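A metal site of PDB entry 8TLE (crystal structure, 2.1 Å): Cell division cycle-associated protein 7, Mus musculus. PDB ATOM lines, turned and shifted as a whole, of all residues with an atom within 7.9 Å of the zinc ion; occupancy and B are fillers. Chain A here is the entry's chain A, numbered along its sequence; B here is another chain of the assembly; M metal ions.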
ATOM      1  N   SER A  30      -1.864  17.742  28.549  1.00  0.00           N
ATOM      2  CA  SER A  30      -1.497  19.154  28.436  1.00  0.00           C
ATOM      3  C   SER A  30      -2.708  20.066  28.613  1.00  0.00           C
ATOM      4  O   SER A  30      -2.551  21.212  29.051  1.00  0.00           O
ATOM      5  CB  SER A  30      -0.828  19.425  27.095  1.00  0.00           C
ATOM      6  OG  SER A  30      -1.728  19.198  26.021  1.00  0.00           O
ATOM      7  N   LYS A  33      -3.900  21.229  32.558  1.00  0.00           N
ATOM      8  CA  LYS A  33      -2.964  22.052  33.307  1.00  0.00           C
ATOM      9  C   LYS A  33      -3.680  23.210  33.987  1.00  0.00           C
ATOM     10  O   LYS A  33      -4.738  23.673  33.537  1.00  0.00           O
ATOM     11  CB  LYS A  33      -1.855  22.588  32.409  1.00  0.00           C
ATOM     12  CG  LYS A  33      -0.860  21.547  31.950  1.00  0.00           C
ATOM     13  CD  LYS A  33       0.242  22.164  31.101  1.00  0.00           C
ATOM     14  CE  LYS A  33       1.281  21.131  30.715  1.00  0.00           C
ATOM     15  NZ  LYS A  33       2.338  21.721  29.856  1.00  0.00           N
ATOM     16  N   THR A  42       7.290  27.581  34.417  1.00  0.00           N
ATOM     17  CA  THR A  42       7.233  27.589  32.959  1.00  0.00           C
ATOM     18  C   THR A  42       8.040  26.425  32.391  1.00  0.00           C
ATOM     19  O   THR A  42       9.218  26.250  32.719  1.00  0.00           O
ATOM     20  CB  THR A  42       7.769  28.918  32.411  1.00  0.00           C
ATOM     21  OG1 THR A  42       6.957  29.994  32.888  1.00  0.00           O
ATOM     22  CG2 THR A  42       7.755  28.905  30.885  1.00  0.00           C
ATOM     23  N   CYS A  43       7.398  25.629  31.542  1.00  0.00           N
ATOM     24  CA  CYS A  43       8.077  24.581  30.808  1.00  0.00           C
ATOM     25  C   CYS A  43       8.872  25.211  29.662  1.00  0.00           C
ATOM     26  O   CYS A  43       8.343  26.024  28.914  1.00  0.00           O
ATOM     27  CB  CYS A  43       7.084  23.558  30.266  1.00  0.00           C
ATOM     28  SG  CYS A  43       7.781  22.339  29.121  1.00  0.00           S
ATOM     29  N   HIS A  44      10.146  24.828  29.542  1.00  0.00           N
ATOM     30  CA  HIS A  44      10.983  25.400  28.500  1.00  0.00           C
ATOM     31  C   HIS A  44      10.457  25.058  27.107  1.00  0.00           C
ATOM     32  O   HIS A  44      10.589  25.858  26.180  1.00  0.00           O
ATOM     33  CB  HIS A  44      12.427  24.925  28.649  1.00  0.00           C
ATOM     34  CG  HIS A  44      13.297  25.257  27.478  1.00  0.00           C
ATOM     35  ND1 HIS A  44      13.623  26.545  27.130  1.00  0.00           N
ATOM     36  CD2 HIS A  44      13.916  24.458  26.569  1.00  0.00           C
ATOM     37  CE1 HIS A  44      14.404  26.530  26.058  1.00  0.00           C
ATOM     38  NE2 HIS A  44      14.590  25.274  25.710  1.00  0.00           N
ATOM     39  N   GLN A  45       9.863  23.874  26.947  1.00  0.00           N
ATOM     40  CA  GLN A  45       9.432  23.410  25.639  1.00  0.00           C
ATOM     41  C   GLN A  45       8.158  24.119  25.179  1.00  0.00           C
ATOM     42  O   GLN A  45       8.147  24.780  24.140  1.00  0.00           O
ATOM     43  CB  GLN A  45       9.233  21.895  25.651  1.00  0.00           C
ATOM     44  CG  GLN A  45       8.980  21.283  24.292  1.00  0.00           C
ATOM     45  CD  GLN A  45      10.255  21.062  23.502  1.00  0.00           C
ATOM     46  OE1 GLN A  45      11.359  21.066  24.054  1.00  0.00           O
ATOM     47  NE2 GLN A  45      10.118  20.871  22.197  1.00  0.00           N
ATOM     48  N   CYS A  46       7.077  23.971  25.941  1.00  0.00           N
ATOM     49  CA  CYS A  46       5.786  24.524  25.548  1.00  0.00           C
ATOM     50  C   CYS A  46       5.585  25.959  26.024  1.00  0.00           C
ATOM     51  O   CYS A  46       4.609  26.596  25.599  1.00  0.00           O
ATOM     52  CB  CYS A  46       4.648  23.643  26.085  1.00  0.00           C
ATOM     53  SG  CYS A  46       4.519  23.586  27.882  1.00  0.00           S
ATOM     54  N   ARG A  47       6.467  26.471  26.882  1.00  0.00           N
ATOM     55  CA  ARG A  47       6.413  27.864  27.351  1.00  0.00           C
ATOM     56  C   ARG A  47       5.064  28.195  27.998  1.00  0.00           C
ATOM     57  O   ARG A  47       4.477  29.241  27.742  1.00  0.00           O
ATOM     58  CB  ARG A  47       6.724  28.829  26.205  1.00  0.00           C
ATOM     59  CG  ARG A  47       8.092  28.579  25.570  1.00  0.00           C
ATOM     60  CD  ARG A  47       8.460  29.642  24.552  1.00  0.00           C
ATOM     61  NE  ARG A  47       7.738  29.503  23.296  1.00  0.00           N
ATOM     62  CZ  ARG A  47       8.168  28.774  22.270  1.00  0.00           C
ATOM     63  NH1 ARG A  47       9.303  28.099  22.331  1.00  0.00           N
ATOM     64  NH2 ARG A  47       7.439  28.739  21.155  1.00  0.00           N
ATOM     65  N   GLN A  48       4.593  27.294  28.845  1.00  0.00           N
ATOM     66  CA  GLN A  48       3.367  27.495  29.624  1.00  0.00           C
ATOM     67  C   GLN A  48       3.710  27.507  31.104  1.00  0.00           C
ATOM     68  O   GLN A  48       4.383  26.599  31.597  1.00  0.00           O
ATOM     69  CB  GLN A  48       2.339  26.405  29.321  1.00  0.00           C
ATOM     70  CG  GLN A  48       2.004  26.247  27.850  1.00  0.00           C
ATOM     71  CD  GLN A  48       1.429  27.521  27.249  1.00  0.00           C
ATOM     72  OE1 GLN A  48       0.302  27.908  27.546  1.00  0.00           O
ATOM     73  NE2 GLN A  48       2.216  28.177  26.402  1.00  0.00           N
ATOM     74  N   THR A  50       2.546  26.802  34.440  1.00  0.00           N
ATOM     75  CA  THR A  50       1.517  26.024  35.092  1.00  0.00           C
ATOM     76  C   THR A  50       2.067  25.430  36.389  1.00  0.00           C
ATOM     77  O   THR A  50       3.266  25.495  36.675  1.00  0.00           O
ATOM     78  CB  THR A  50       0.989  24.904  34.179  1.00  0.00           C
ATOM     79  OG1 THR A  50       2.073  24.026  33.836  1.00  0.00           O
ATOM     80  CG2 THR A  50       0.398  25.484  32.907  1.00  0.00           C
ATOM     81  N   ASP A  52       1.862  22.175  37.429  1.00  0.00           N
ATOM     82  CA  ASP A  52       2.244  20.773  37.454  1.00  0.00           C
ATOM     83  C   ASP A  52       3.741  20.631  37.692  1.00  0.00           C
ATOM     84  O   ASP A  52       4.534  21.538  37.431  1.00  0.00           O
ATOM     85  CB  ASP A  52       1.856  20.087  36.144  1.00  0.00           C
ATOM     86  CG  ASP A  52       2.389  20.819  34.923  1.00  0.00           C
ATOM     87  OD1 ASP A  52       2.097  22.027  34.800  1.00  0.00           O
ATOM     88  OD2 ASP A  52       3.090  20.199  34.103  1.00  0.00           O
ATOM     89  N   LYS A  54       7.532  19.724  37.247  1.00  0.00           N
ATOM     90  CA  LYS A  54       8.391  19.789  36.075  1.00  0.00           C
ATOM     91  C   LYS A  54       9.816  19.386  36.459  1.00  0.00           C
ATOM     92  O   LYS A  54      10.182  19.357  37.631  1.00  0.00           O
ATOM     93  CB  LYS A  54       8.382  21.201  35.459  1.00  0.00           C
ATOM     94  CG  LYS A  54       6.999  21.642  35.020  1.00  0.00           C
ATOM     95  CD  LYS A  54       7.027  22.980  34.302  1.00  0.00           C
ATOM     96  CE  LYS A  54       5.631  23.360  33.830  1.00  0.00           C
ATOM     97  NZ  LYS A  54       4.686  23.513  34.979  1.00  0.00           N
ATOM     98  N   GLN A  68      13.540  23.208  32.863  1.00  0.00           N
ATOM     99  CA  GLN A  68      12.217  22.833  33.367  1.00  0.00           C
ATOM    100  C   GLN A  68      11.358  22.350  32.208  1.00  0.00           C
ATOM    101  O   GLN A  68      11.069  23.122  31.281  1.00  0.00           O
ATOM    102  CB  GLN A  68      11.561  24.008  34.083  1.00  0.00           C
ATOM    103  CG  GLN A  68      12.348  24.548  35.256  1.00  0.00           C
ATOM    104  CD  GLN A  68      11.697  25.766  35.893  1.00  0.00           C
ATOM    105  OE1 GLN A  68      10.650  26.231  35.435  1.00  0.00           O
ATOM    106  NE2 GLN A  68      12.317  26.298  36.933  1.00  0.00           N
ATOM    107  N   PHE A  69      10.943  21.087  32.260  1.00  0.00           N
ATOM    108  CA  PHE A  69      10.103  20.489  31.242  1.00  0.00           C
ATOM    109  C   PHE A  69       8.903  19.820  31.895  1.00  0.00           C
ATOM    110  O   PHE A  69       9.045  19.143  32.914  1.00  0.00           O
ATOM    111  CB  PHE A  69      10.876  19.467  30.399  1.00  0.00           C
ATOM    112  CG  PHE A  69      11.897  20.085  29.487  1.00  0.00           C
ATOM    113  CD1 PHE A  69      13.114  20.529  29.972  1.00  0.00           C
ATOM    114  CD2 PHE A  69      11.631  20.235  28.132  1.00  0.00           C
ATOM    115  CE1 PHE A  69      14.046  21.101  29.133  1.00  0.00           C
ATOM    116  CE2 PHE A  69      12.555  20.799  27.280  1.00  0.00           C
ATOM    117  CZ  PHE A  69      13.767  21.236  27.780  1.00  0.00           C
ATOM    118  N   CYS A  70       7.729  20.002  31.298  1.00  0.00           N
ATOM    119  CA  CYS A  70       6.503  19.428  31.831  1.00  0.00           C
ATOM    120  C   CYS A  70       6.411  17.948  31.442  1.00  0.00           C
ATOM    121  O   CYS A  70       7.270  17.400  30.747  1.00  0.00           O
ATOM    122  CB  CYS A  70       5.292  20.196  31.328  1.00  0.00           C
ATOM    123  SG  CYS A  70       4.973  20.032  29.550  1.00  0.00           S
ATOM    124  N   GLY A  71       5.342  17.299  31.904  1.00  0.00           N
ATOM    125  CA  GLY A  71       5.110  15.897  31.634  1.00  0.00           C
ATOM    126  C   GLY A  71       4.952  15.597  30.162  1.00  0.00           C
ATOM    127  O   GLY A  71       5.744  14.847  29.576  1.00  0.00           O
ATOM    128  N   PRO A  72       3.907  16.151  29.525  1.00  0.00           N
ATOM    129  CA  PRO A  72       3.685  15.863  28.101  1.00  0.00           C
ATOM    130  C   PRO A  72       4.854  16.245  27.206  1.00  0.00           C
ATOM    131  O   PRO A  72       5.139  15.535  26.229  1.00  0.00           O
ATOM    132  CB  PRO A  72       2.434  16.676  27.772  1.00  0.00           C
ATOM    133  CG  PRO A  72       1.715  16.795  29.077  1.00  0.00           C
ATOM    134  CD  PRO A  72       2.795  16.916  30.114  1.00  0.00           C
ATOM    135  N   CYS A  73       5.537  17.358  27.493  1.00  0.00           N
ATOM    136  CA  CYS A  73       6.618  17.811  26.606  1.00  0.00           C
ATOM    137  C   CYS A  73       7.803  16.864  26.638  1.00  0.00           C
ATOM    138  O   CYS A  73       8.309  16.461  25.585  1.00  0.00           O
ATOM    139  CB  CYS A  73       7.038  19.225  26.978  1.00  0.00           C
ATOM    140  SG  CYS A  73       5.998  20.516  26.266  1.00  0.00           S
ATOM    141  N   LEU A  74       8.265  16.482  27.834  1.00  0.00           N
ATOM    142  CA  LEU A  74       9.374  15.544  27.923  1.00  0.00           C
ATOM    143  C   LEU A  74       8.970  14.169  27.414  1.00  0.00           C
ATOM    144  O   LEU A  74       9.804  13.450  26.844  1.00  0.00           O
ATOM    145  CB  LEU A  74       9.868  15.449  29.361  1.00  0.00           C
ATOM    146  CG  LEU A  74      11.212  14.743  29.566  1.00  0.00           C
ATOM    147  CD1 LEU A  74      12.353  15.560  28.980  1.00  0.00           C
ATOM    148  CD2 LEU A  74      11.460  14.443  31.038  1.00  0.00           C
ATOM    149  N   ARG A  77       8.439  14.874  23.214  1.00  0.00           N
ATOM    150  CA  ARG A  77       9.533  15.454  22.451  1.00  0.00           C
ATOM    151  C   ARG A  77      10.867  14.745  22.678  1.00  0.00           C
ATOM    152  O   ARG A  77      11.798  14.935  21.881  1.00  0.00           O
ATOM    153  CB  ARG A  77       9.689  16.935  22.785  1.00  0.00           C
ATOM    154  CG  ARG A  77       8.412  17.747  22.614  1.00  0.00           C
ATOM    155  CD  ARG A  77       8.003  17.840  21.147  1.00  0.00           C
ATOM    156  NE  ARG A  77       8.987  18.563  20.358  1.00  0.00           N
ATOM    157  CZ  ARG A  77       8.782  19.029  19.135  1.00  0.00           C
ATOM    158  NH1 ARG A  77       7.610  18.877  18.535  1.00  0.00           N
ATOM    159  NH2 ARG A  77       9.757  19.667  18.504  1.00  0.00           N
ATOM    160  P    DT B  13       4.120  18.192  20.891  1.00  0.00           P
ATOM    161  OP1  DT B  13       5.051  17.559  19.920  1.00  0.00           O
ATOM    162  OP2  DT B  13       4.463  18.228  22.328  1.00  0.00           O
ATOM    163  O5'  DT B  13       3.832  19.691  20.415  1.00  0.00           O
ATOM    164  C5'  DT B  13       3.513  19.960  19.057  1.00  0.00           C
ATOM    165  C4'  DT B  13       3.242  21.443  18.842  1.00  0.00           C
ATOM    166  O4'  DT B  13       2.147  21.845  19.683  1.00  0.00           O
ATOM    167  C3'  DT B  13       4.387  22.362  19.236  1.00  0.00           C
ATOM    168  O3'  DT B  13       5.277  22.504  18.137  1.00  0.00           O
ATOM    169  C2'  DT B  13       3.666  23.680  19.537  1.00  0.00           C
ATOM    170  C1'  DT B  13       2.280  23.210  20.014  1.00  0.00           C
ATOM    171  N1   DT B  13       2.052  23.377  21.469  1.00  0.00           N
ATOM    172  C2   DT B  13       1.700  24.612  21.962  1.00  0.00           C
ATOM    173  O2   DT B  13       1.569  25.590  21.258  1.00  0.00           O
ATOM    174  N3   DT B  13       1.509  24.663  23.316  1.00  0.00           N
ATOM    175  C4   DT B  13       1.636  23.612  24.214  1.00  0.00           C
ATOM    176  O4   DT B  13       1.440  23.763  25.418  1.00  0.00           O
ATOM    177  C5   DT B  13       2.010  22.347  23.634  1.00  0.00           C
ATOM    178  C7   DT B  13       2.169  21.138  24.509  1.00  0.00           C
ATOM    179  C6   DT B  13       2.196  22.289  22.309  1.00  0.00           C
HETATM  180 ZN    ZN M   1       5.758  21.689  28.206  1.00  0.00          ZN
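Merely in contact with the zinc ion: Lys 33 (3.8 Å).
SG of Cys 70 lies close to NZ of Lys 33 (3.1 Å). The side-chain sulfur of Cys 46 sits close to the side-chain amino group of Lys 33 (3.5 Å). O of Cys 46 sits at hydrogen-bond distance from NE2 of Gln 48, at 3.0 Å. N of Gln 45 sits close to SG of Cys 43 (3.4 Å). The backbone carbonyl oxygen (O) of Gln 48 sits at hydrogen-bond distance from the backbone NH (N) of Cys 43 (3.2 Å).
The zinc ion is bound by the side-chain sulfur (SG) of Cys 70 (2.3 Å), the side-chain sulfur (SG) of Cys 73 (2.3 Å), the side-chain sulfur (SG) of Cys 46 (2.3 Å) and the side-chain sulfur (SG) of Cys 43 (2.3 Å). The zinc ion has four donor atoms within binding distance.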
